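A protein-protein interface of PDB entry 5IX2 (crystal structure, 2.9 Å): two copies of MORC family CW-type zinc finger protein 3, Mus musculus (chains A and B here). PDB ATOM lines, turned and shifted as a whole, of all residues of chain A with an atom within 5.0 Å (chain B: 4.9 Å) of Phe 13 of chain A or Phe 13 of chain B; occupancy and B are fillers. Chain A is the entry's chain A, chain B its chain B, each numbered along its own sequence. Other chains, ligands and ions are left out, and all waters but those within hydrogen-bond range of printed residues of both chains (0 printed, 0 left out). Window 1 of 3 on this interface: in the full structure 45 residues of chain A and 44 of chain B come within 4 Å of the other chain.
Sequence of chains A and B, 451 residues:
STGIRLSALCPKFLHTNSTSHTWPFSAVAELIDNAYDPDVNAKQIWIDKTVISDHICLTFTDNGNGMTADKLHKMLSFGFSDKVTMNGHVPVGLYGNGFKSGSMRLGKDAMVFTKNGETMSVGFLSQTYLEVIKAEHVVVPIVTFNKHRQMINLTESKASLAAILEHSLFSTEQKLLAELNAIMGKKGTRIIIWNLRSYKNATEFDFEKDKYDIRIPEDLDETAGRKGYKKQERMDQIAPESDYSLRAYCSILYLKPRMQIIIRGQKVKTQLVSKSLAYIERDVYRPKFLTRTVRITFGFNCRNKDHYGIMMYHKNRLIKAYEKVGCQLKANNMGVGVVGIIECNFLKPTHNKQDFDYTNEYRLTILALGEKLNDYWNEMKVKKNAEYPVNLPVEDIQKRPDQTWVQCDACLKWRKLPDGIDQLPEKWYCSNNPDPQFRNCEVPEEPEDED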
ATOM      1  N   LEU A   9      -5.032  18.882  10.318  1.00  0.00           N
ATOM      2  CA  LEU A   9      -6.462  18.716  10.230  1.00  0.00           C
ATOM      3  C   LEU A   9      -7.074  19.716  11.127  1.00  0.00           C
ATOM      4  O   LEU A   9      -6.669  19.877  12.236  1.00  0.00           O
ATOM      5  CB  LEU A   9      -6.857  17.361  10.738  1.00  0.00           C
ATOM      6  CG  LEU A   9      -7.439  16.336   9.803  1.00  0.00           C
ATOM      7  CD1 LEU A   9      -8.015  16.985   8.576  1.00  0.00           C
ATOM      8  CD2 LEU A   9      -6.365  15.352   9.430  1.00  0.00           C
ATOM      9  N   CYS A  10      -8.077  20.390  10.639  1.00  0.00           N
ATOM     10  CA  CYS A  10      -8.680  21.457  11.361  1.00  0.00           C
ATOM     11  C   CYS A  10      -9.999  20.925  11.785  1.00  0.00           C
ATOM     12  O   CYS A  10     -10.630  20.231  11.017  1.00  0.00           O
ATOM     13  CB  CYS A  10      -8.871  22.618  10.422  1.00  0.00           C
ATOM     14  SG  CYS A  10      -9.505  24.112  11.149  1.00  0.00           S
ATOM     15  N   PRO A  11     -10.424  21.278  13.076  1.00  0.00           N
ATOM     16  CA  PRO A  11     -11.707  20.678  13.445  1.00  0.00           C
ATOM     17  C   PRO A  11     -12.772  21.027  12.459  1.00  0.00           C
ATOM     18  O   PRO A  11     -13.684  20.279  12.269  1.00  0.00           O
ATOM     19  CB  PRO A  11     -12.034  21.304  14.796  1.00  0.00           C
ATOM     20  CG  PRO A  11     -11.131  22.432  14.975  1.00  0.00           C
ATOM     21  CD  PRO A  11      -9.896  21.952  14.357  1.00  0.00           C
ATOM     22  N   LYS A  12     -12.650  22.157  11.815  1.00  0.00           N
ATOM     23  CA  LYS A  12     -13.645  22.576  10.847  1.00  0.00           C
ATOM     24  C   LYS A  12     -13.797  21.595   9.711  1.00  0.00           C
ATOM     25  O   LYS A  12     -14.842  21.483   9.129  1.00  0.00           O
ATOM     26  CB  LYS A  12     -13.258  23.921  10.293  1.00  0.00           C
ATOM     27  CG  LYS A  12     -14.299  24.558   9.414  1.00  0.00           C
ATOM     28  CD  LYS A  12     -13.743  25.832   8.822  1.00  0.00           C
ATOM     29  CE  LYS A  12     -13.266  26.752   9.917  1.00  0.00           C
ATOM     30  NZ  LYS A  12     -13.226  28.154   9.456  1.00  0.00           N
ATOM     31  N   PHE A  13     -12.735  20.893   9.390  1.00  0.00           N
ATOM     32  CA  PHE A  13     -12.760  19.987   8.277  1.00  0.00           C
ATOM     33  C   PHE A  13     -13.789  18.931   8.499  1.00  0.00           C
ATOM     34  O   PHE A  13     -14.295  18.361   7.568  1.00  0.00           O
ATOM     35  CB  PHE A  13     -11.424  19.311   8.099  1.00  0.00           C
ATOM     36  CG  PHE A  13     -11.368  18.414   6.911  1.00  0.00           C
ATOM     37  CD1 PHE A  13     -11.584  18.898   5.662  1.00  0.00           C
ATOM     38  CD2 PHE A  13     -11.111  17.090   7.061  1.00  0.00           C
ATOM     39  CE1 PHE A  13     -11.533  18.081   4.577  1.00  0.00           C
ATOM     40  CE2 PHE A  13     -11.060  16.261   5.987  1.00  0.00           C
ATOM     41  CZ  PHE A  13     -11.272  16.759   4.741  1.00  0.00           C
ATOM     42  N   LEU A  14     -14.069  18.632   9.743  1.00  0.00           N
ATOM     43  CA  LEU A  14     -14.935  17.522  10.055  1.00  0.00           C
ATOM     44  C   LEU A  14     -16.297  17.707   9.457  1.00  0.00           C
ATOM     45  O   LEU A  14     -16.925  16.763   9.047  1.00  0.00           O
ATOM     46  CB  LEU A  14     -15.054  17.363  11.556  1.00  0.00           C
ATOM     47  CG  LEU A  14     -13.907  16.699  12.293  1.00  0.00           C
ATOM     48  CD1 LEU A  14     -14.119  16.875  13.767  1.00  0.00           C
ATOM     49  CD2 LEU A  14     -13.817  15.237  11.960  1.00  0.00           C
ATOM     50  N   HIS A  15     -16.782  18.927   9.474  1.00  0.00           N
ATOM     51  CA  HIS A  15     -18.017  19.261   8.811  1.00  0.00           C
ATOM     52  C   HIS A  15     -17.917  19.106   7.326  1.00  0.00           C
ATOM     53  O   HIS A  15     -18.835  18.691   6.670  1.00  0.00           O
ATOM     54  CB  HIS A  15     -18.385  20.695   9.098  1.00  0.00           C
ATOM     55  CG  HIS A  15     -19.598  21.147   8.369  1.00  0.00           C
ATOM     56  ND1 HIS A  15     -20.615  20.289   8.048  1.00  0.00           N
ATOM     57  CD2 HIS A  15     -19.933  22.339   7.847  1.00  0.00           C
ATOM     58  CE1 HIS A  15     -21.551  20.944   7.397  1.00  0.00           C
ATOM     59  NE2 HIS A  15     -21.154  22.188   7.250  1.00  0.00           N
ATOM     60  N   THR A  16     -16.799  19.524   6.800  1.00  0.00           N
ATOM     61  CA  THR A  16     -16.649  19.637   5.395  1.00  0.00           C
ATOM     62  C   THR A  16     -16.808  18.271   4.832  1.00  0.00           C
ATOM     63  O   THR A  16     -17.498  18.079   3.865  1.00  0.00           O
ATOM     64  CB  THR A  16     -15.276  20.196   5.086  1.00  0.00           C
ATOM     65  OG1 THR A  16     -15.230  21.538   5.545  1.00  0.00           O
ATOM     66  CG2 THR A  16     -15.048  20.188   3.654  1.00  0.00           C
ATOM     67  N   ASN A  17     -16.223  17.303   5.493  1.00  0.00           N
ATOM     68  CA  ASN A  17     -16.175  15.975   4.971  1.00  0.00           C
ATOM     69  C   ASN A  17     -17.549  15.397   4.844  1.00  0.00           C
ATOM     70  O   ASN A  17     -17.747  14.446   4.151  1.00  0.00           O
ATOM     71  CB  ASN A  17     -15.311  15.106   5.835  1.00  0.00           C
ATOM     72  CG  ASN A  17     -14.568  14.083   5.050  1.00  0.00           C
ATOM     73  OD1 ASN A  17     -14.633  12.905   5.327  1.00  0.00           O
ATOM     74  ND2 ASN A  17     -13.848  14.528   4.067  1.00  0.00           N
ATOM     75  N   PHE A  78      -8.114   9.885   9.160  1.00  0.00           N
ATOM     76  CA  PHE A  78      -8.578   9.867   7.784  1.00  0.00           C
ATOM     77  C   PHE A  78      -7.682   9.156   6.812  1.00  0.00           C
ATOM     78  O   PHE A  78      -6.516   9.417   6.729  1.00  0.00           O
ATOM     79  CB  PHE A  78      -8.763  11.266   7.272  1.00  0.00           C
ATOM     80  CG  PHE A  78      -9.680  12.085   8.080  1.00  0.00           C
ATOM     81  CD1 PHE A  78     -10.965  12.248   7.710  1.00  0.00           C
ATOM     82  CD2 PHE A  78      -9.235  12.714   9.185  1.00  0.00           C
ATOM     83  CE1 PHE A  78     -11.805  13.023   8.444  1.00  0.00           C
ATOM     84  CE2 PHE A  78     -10.060  13.498   9.918  1.00  0.00           C
ATOM     85  CZ  PHE A  78     -11.351  13.650   9.552  1.00  0.00           C
ATOM     86  N   GLY A  79      -8.280   8.288   6.032  1.00  0.00           N
ATOM     87  CA  GLY A  79      -7.589   7.600   4.982  1.00  0.00           C
ATOM     88  C   GLY A  79      -6.970   6.269   5.254  1.00  0.00           C
ATOM     89  O   GLY A  79      -6.362   5.709   4.379  1.00  0.00           O
ATOM     90  N   TYR A  95     -11.841   3.542   1.013  1.00  0.00           N
ATOM     91  CA  TYR A  95     -11.388   4.943   1.106  1.00  0.00           C
ATOM     92  C   TYR A  95     -10.883   5.441   2.451  1.00  0.00           C
ATOM     93  O   TYR A  95     -10.245   6.490   2.525  1.00  0.00           O
ATOM     94  CB  TYR A  95     -12.525   5.880   0.697  1.00  0.00           C
ATOM     95  CG  TYR A  95     -12.941   5.754  -0.741  1.00  0.00           C
ATOM     96  CD1 TYR A  95     -12.002   5.509  -1.741  1.00  0.00           C
ATOM     97  CD2 TYR A  95     -14.271   5.874  -1.108  1.00  0.00           C
ATOM     98  CE1 TYR A  95     -12.386   5.386  -3.069  1.00  0.00           C
ATOM     99  CE2 TYR A  95     -14.658   5.758  -2.440  1.00  0.00           C
ATOM    100  CZ  TYR A  95     -13.715   5.514  -3.407  1.00  0.00           C
ATOM    101  OH  TYR A  95     -14.118   5.384  -4.710  1.00  0.00           O
ATOM    102  N   ASN A  97     -12.672   6.650   4.838  1.00  0.00           N
ATOM    103  CA  ASN A  97     -13.304   7.925   5.163  1.00  0.00           C
ATOM    104  C   ASN A  97     -14.735   7.816   5.664  1.00  0.00           C
ATOM    105  O   ASN A  97     -15.257   8.727   6.311  1.00  0.00           O
ATOM    106  CB  ASN A  97     -13.268   8.836   3.937  1.00  0.00           C
ATOM    107  CG  ASN A  97     -13.795  10.211   4.229  1.00  0.00           C
ATOM    108  OD1 ASN A  97     -14.623  10.738   3.487  1.00  0.00           O
ATOM    109  ND2 ASN A  97     -13.336  10.800   5.328  1.00  0.00           N
ATOM    110  N   LEU B   9      -3.741  11.830   8.839  1.00  0.00           N
ATOM    111  CA  LEU B   9      -4.076  11.736   7.434  1.00  0.00           C
ATOM    112  C   LEU B   9      -3.210  10.760   6.722  1.00  0.00           C
ATOM    113  O   LEU B   9      -2.024  10.892   6.672  1.00  0.00           O
ATOM    114  CB  LEU B   9      -3.873  13.065   6.757  1.00  0.00           C
ATOM    115  CG  LEU B   9      -4.817  14.184   7.101  1.00  0.00           C
ATOM    116  CD1 LEU B   9      -4.080  15.473   6.902  1.00  0.00           C
ATOM    117  CD2 LEU B   9      -6.013  14.124   6.195  1.00  0.00           C
ATOM    118  N   CYS B  10      -3.838   9.790   6.119  1.00  0.00           N
ATOM    119  CA  CYS B  10      -3.147   8.843   5.313  1.00  0.00           C
ATOM    120  C   CYS B  10      -2.920   9.450   3.962  1.00  0.00           C
ATOM    121  O   CYS B  10      -3.754  10.181   3.471  1.00  0.00           O
ATOM    122  CB  CYS B  10      -3.999   7.608   5.189  1.00  0.00           C
ATOM    123  SG  CYS B  10      -3.122   6.166   4.644  1.00  0.00           S
ATOM    124  N   PRO B  11      -1.742   9.056   3.320  1.00  0.00           N
ATOM    125  CA  PRO B  11      -1.621   9.552   1.956  1.00  0.00           C
ATOM    126  C   PRO B  11      -2.793   9.131   1.128  1.00  0.00           C
ATOM    127  O   PRO B  11      -3.150   9.792   0.192  1.00  0.00           O
ATOM    128  CB  PRO B  11      -0.406   8.818   1.450  1.00  0.00           C
ATOM    129  CG  PRO B  11       0.506   8.883   2.583  1.00  0.00           C
ATOM    130  CD  PRO B  11      -0.386   8.381   3.641  1.00  0.00           C
ATOM    131  N   LYS B  12      -3.375   8.007   1.447  1.00  0.00           N
ATOM    132  CA  LYS B  12      -4.423   7.450   0.638  1.00  0.00           C
ATOM    133  C   LYS B  12      -5.582   8.390   0.581  1.00  0.00           C
ATOM    134  O   LYS B  12      -6.351   8.359  -0.327  1.00  0.00           O
ATOM    135  CB  LYS B  12      -4.847   6.144   1.243  1.00  0.00           C
ATOM    136  CG  LYS B  12      -5.672   5.255   0.359  1.00  0.00           C
ATOM    137  CD  LYS B  12      -5.953   3.952   1.076  1.00  0.00           C
ATOM    138  CE  LYS B  12      -4.687   3.137   1.240  1.00  0.00           C
ATOM    139  NZ  LYS B  12      -4.985   1.754   1.670  1.00  0.00           N
ATOM    140  N   PHE B  13      -5.697   9.245   1.565  1.00  0.00           N
ATOM    141  CA  PHE B  13      -6.794  10.184   1.627  1.00  0.00           C
ATOM    142  C   PHE B  13      -6.792  11.166   0.466  1.00  0.00           C
ATOM    143  O   PHE B  13      -7.828  11.608   0.001  1.00  0.00           O
ATOM    144  CB  PHE B  13      -6.792  10.921   2.952  1.00  0.00           C
ATOM    145  CG  PHE B  13      -8.072  11.620   3.244  1.00  0.00           C
ATOM    146  CD1 PHE B  13      -9.248  10.952   3.189  1.00  0.00           C
ATOM    147  CD2 PHE B  13      -8.087  12.943   3.536  1.00  0.00           C
ATOM    148  CE1 PHE B  13     -10.420  11.587   3.438  1.00  0.00           C
ATOM    149  CE2 PHE B  13      -9.252  13.585   3.786  1.00  0.00           C
ATOM    150  CZ  PHE B  13     -10.420  12.906   3.735  1.00  0.00           C
ATOM    151  N   LEU B  14      -5.615  11.523   0.004  1.00  0.00           N
ATOM    152  CA  LEU B  14      -5.500  12.572  -0.974  1.00  0.00           C
ATOM    153  C   LEU B  14      -6.305  12.177  -2.176  1.00  0.00           C
ATOM    154  O   LEU B  14      -6.927  13.003  -2.788  1.00  0.00           O
ATOM    155  CB  LEU B  14      -4.054  12.782  -1.360  1.00  0.00           C
ATOM    156  CG  LEU B  14      -3.187  13.447  -0.320  1.00  0.00           C
ATOM    157  CD1 LEU B  14      -1.766  13.420  -0.790  1.00  0.00           C
ATOM    158  CD2 LEU B  14      -3.629  14.863  -0.091  1.00  0.00           C
ATOM    159  N   HIS B  15      -6.274  10.916  -2.530  1.00  0.00           N
ATOM    160  CA  HIS B  15      -7.146  10.417  -3.553  1.00  0.00           C
ATOM    161  C   HIS B  15      -8.580  10.472  -3.143  1.00  0.00           C
ATOM    162  O   HIS B  15      -9.439  10.631  -3.964  1.00  0.00           O
ATOM    163  CB  HIS B  15      -6.794   9.009  -3.954  1.00  0.00           C
ATOM    164  CG  HIS B  15      -7.745   8.424  -4.936  1.00  0.00           C
ATOM    165  ND1 HIS B  15      -8.324   9.168  -5.927  1.00  0.00           N
ATOM    166  CD2 HIS B  15      -8.253   7.184  -5.056  1.00  0.00           C
ATOM    167  CE1 HIS B  15      -9.127   8.407  -6.637  1.00  0.00           C
ATOM    168  NE2 HIS B  15      -9.112   7.199  -6.120  1.00  0.00           N
ATOM    169  N   THR B  16      -8.844  10.202  -1.887  1.00  0.00           N
ATOM    170  CA  THR B  16     -10.204  10.142  -1.424  1.00  0.00           C
ATOM    171  C   THR B  16     -10.891  11.469  -1.520  1.00  0.00           C
ATOM    172  O   THR B  16     -12.005  11.527  -1.962  1.00  0.00           O
ATOM    173  CB  THR B  16     -10.309   9.554  -0.027  1.00  0.00           C
ATOM    174  OG1 THR B  16      -9.764   8.247  -0.048  1.00  0.00           O
ATOM    175  CG2 THR B  16     -11.707   9.440   0.334  1.00  0.00           C
ATOM    176  N   ASN B  17     -10.217  12.546  -1.171  1.00  0.00           N
ATOM    177  CA  ASN B  17     -10.874  13.837  -1.135  1.00  0.00           C
ATOM    178  C   ASN B  17     -11.357  14.198  -2.513  1.00  0.00           C
ATOM    179  O   ASN B  17     -12.262  14.973  -2.689  1.00  0.00           O
ATOM    180  CB  ASN B  17      -9.965  14.920  -0.594  1.00  0.00           C
ATOM    181  CG  ASN B  17     -10.550  15.607   0.600  1.00  0.00           C
ATOM    182  OD1 ASN B  17      -9.845  16.063   1.481  1.00  0.00           O
ATOM    183  ND2 ASN B  17     -11.853  15.688   0.632  1.00  0.00           N
ATOM    184  N   PHE B  78      -5.656  20.367   5.535  1.00  0.00           N
ATOM    185  CA  PHE B  78      -7.102  20.313   5.412  1.00  0.00           C
ATOM    186  C   PHE B  78      -7.868  21.068   6.452  1.00  0.00           C
ATOM    187  O   PHE B  78      -7.572  20.996   7.600  1.00  0.00           O
ATOM    188  CB  PHE B  78      -7.589  18.896   5.438  1.00  0.00           C
ATOM    189  CG  PHE B  78      -6.891  18.020   4.487  1.00  0.00           C
ATOM    190  CD1 PHE B  78      -5.569  17.803   4.603  1.00  0.00           C
ATOM    191  CD2 PHE B  78      -7.566  17.407   3.496  1.00  0.00           C
ATOM    192  CE1 PHE B  78      -4.914  16.990   3.739  1.00  0.00           C
ATOM    193  CE2 PHE B  78      -6.924  16.582   2.631  1.00  0.00           C
ATOM    194  CZ  PHE B  78      -5.594  16.373   2.752  1.00  0.00           C
ATOM    195  N   GLY B  79      -8.877  21.779   6.004  1.00  0.00           N
ATOM    196  CA  GLY B  79      -9.816  22.461   6.847  1.00  0.00           C
ATOM    197  C   GLY B  79      -9.588  23.890   7.216  1.00  0.00           C
ATOM    198  O   GLY B  79     -10.461  24.502   7.774  1.00  0.00           O
ATOM    199  N   ASN B  97     -11.221  22.960   1.787  1.00  0.00           N
ATOM    200  CA  ASN B  97     -10.799  21.760   1.097  1.00  0.00           C
ATOM    201  C   ASN B  97     -10.512  21.868  -0.389  1.00  0.00           C
ATOM    202  O   ASN B  97      -9.929  20.980  -0.963  1.00  0.00           O
ATOM    203  CB  ASN B  97     -11.853  20.698   1.299  1.00  0.00           C
ATOM    204  CG  ASN B  97     -11.429  19.372   0.795  1.00  0.00           C
ATOM    205  OD1 ASN B  97     -12.213  18.644   0.255  1.00  0.00           O
ATOM    206  ND2 ASN B  97     -10.184  19.058   0.963  1.00  0.00           N
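Phe 13 of chain A touches just these residues of chain B: Phe 13, Asn 17, Phe 78, Gly 79 and Asn 97. Thr 16 of chain A touches none of the printed residues of chain B. Printed residues of chain B within 4 Å of Asn 17 of chain A: Phe 13 (3.8 Å). Of the printed residues of chain B, Asn 97 of chain A touches Phe 13 and Thr 16. Of the printed residues of chain A, Lys 12 of chain B touches Gly 79. Phe 13 of chain B touches four residues of chain A. Leu 14 of chain B touches none of the printed residues of chain A. Of the printed residues of chain A, Asn 17 of chain B touches Phe 13 (3.6 Å). The nearest printed residue of chain B that does not touch Phe 13 of chain A is Leu 9 of chain B (5.5 Å). The nearest residue of chain A that does not touch Phe 13 of chain B is Phe 78 of chain A (4.1 Å).
The backbone NH (N) of Lys 12 of chain B lies close to the side-chain sulfur (SG) of Cys 10 of chain B (3.7 Å). The side-chain amide oxygen (OD1) of Asn 97 of chain B lies within hydrogen-bond range of the side-chain amide nitrogen (ND2) of Asn 17 of chain B (3.0 Å). SG of Cys 10 of chain A sits close to N of Lys 12 of chain A (3.8 Å). The side-chain amide oxygen of Asn 17 of chain A sits at hydrogen-bond distance from the side-chain amide nitrogen of Asn 97 of chain A, 2.5 Å away. The backbone carbonyl oxygen (O) of Lys 12 of chain B sits at hydrogen-bond distance from the side-chain hydroxyl (OG1) of Thr 16 of chain B (3.4 Å).
Of the 12 printed residues of chain B, 9 touch a printed residue of chain A. Hydrophobic or aromatic side chains of chain A that line the printed part of chain B: Leu 9, Phe 13 and Tyr 95. Among the printed residues, 19 pairs touch across the chains. Among the printed residues, no Asp or Glu carboxylate lies within 4 Å of a Lys or Arg side-chain nitrogen of the other chain.
Leu 9 of chain B touches its own counterpart, Leu 9 of chain A. Cys 10 of chain A touches Gly 79 of chain B, and with the chains exchanged Gly 79 of chain A touches Cys 10 of chain B. Lys 12 of chain A touches Gly 79 of chain B, and with the chains exchanged Gly 79 of chain A touches Lys 12 of chain B. Phe 13 of chain A touches its own counterpart, Phe 13 of chain B. Of the 19 pairs that touch across the chains among the printed residues, 16 have their exchanged pair printed and touching as well.
Among the printed residues, merely in contact across the chains: Leu 9 of chain A with Leu 9 of chain B (3.0 Å), Phe 78 of chain A with Leu 9 of chain B (3.4 Å), Gly 79 of chain A with Lys 12 of chain B (3.5 Å), Asn 97 of chain A with Phe 13 of chain B (3.6 Å), Phe 13 of chain A with Asn 17 of chain B (3.6 Å), Leu 9 of chain A with Phe 78 of chain B (3.7 Å), Lys 12 of chain A with Gly 79 of chain B (3.7 Å), Phe 13 of chain A with Gly 79 of chain B (3.8 Å), Asn 17 of chain A with Phe 13 of chain B (3.8 Å), Phe 13 of chain A with Phe 13 of chain B (3.9 Å), Phe 13 of chain A with Phe 78 of chain B (3.96 Å), Asn 97 of chain A with Thr 16 of chain B (3.97 Å), Gly 79 of chain A with Phe 13 of chain B (3.97 Å) and Phe 13 of chain A with Asn 97 of chain B (3.98 Å).
The side-chain sulfur (SG) of Cys 10 of chain B sits close to the backbone carbonyl oxygen (O) of Gly 79 of chain A (3.3 Å). The backbone carbonyl oxygen of Phe 78 of chain B is in hydrogen-bond range of the backbone NH of Cys 10 of chain A. OG1 of Thr 16 of chain B lies within hydrogen-bond range of O of Tyr 95 of chain A (3.2 Å). The backbone NH (N) of Cys 10 of chain B sits at hydrogen-bond distance from the backbone carbonyl oxygen (O) of Phe 78 of chain A, at 2.8 Å. The backbone carbonyl oxygen (O) of Gly 79 of chain B lies within hydrogen-bond range of the side-chain sulfur (SG) of Cys 10 of chain A (3.5 Å).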
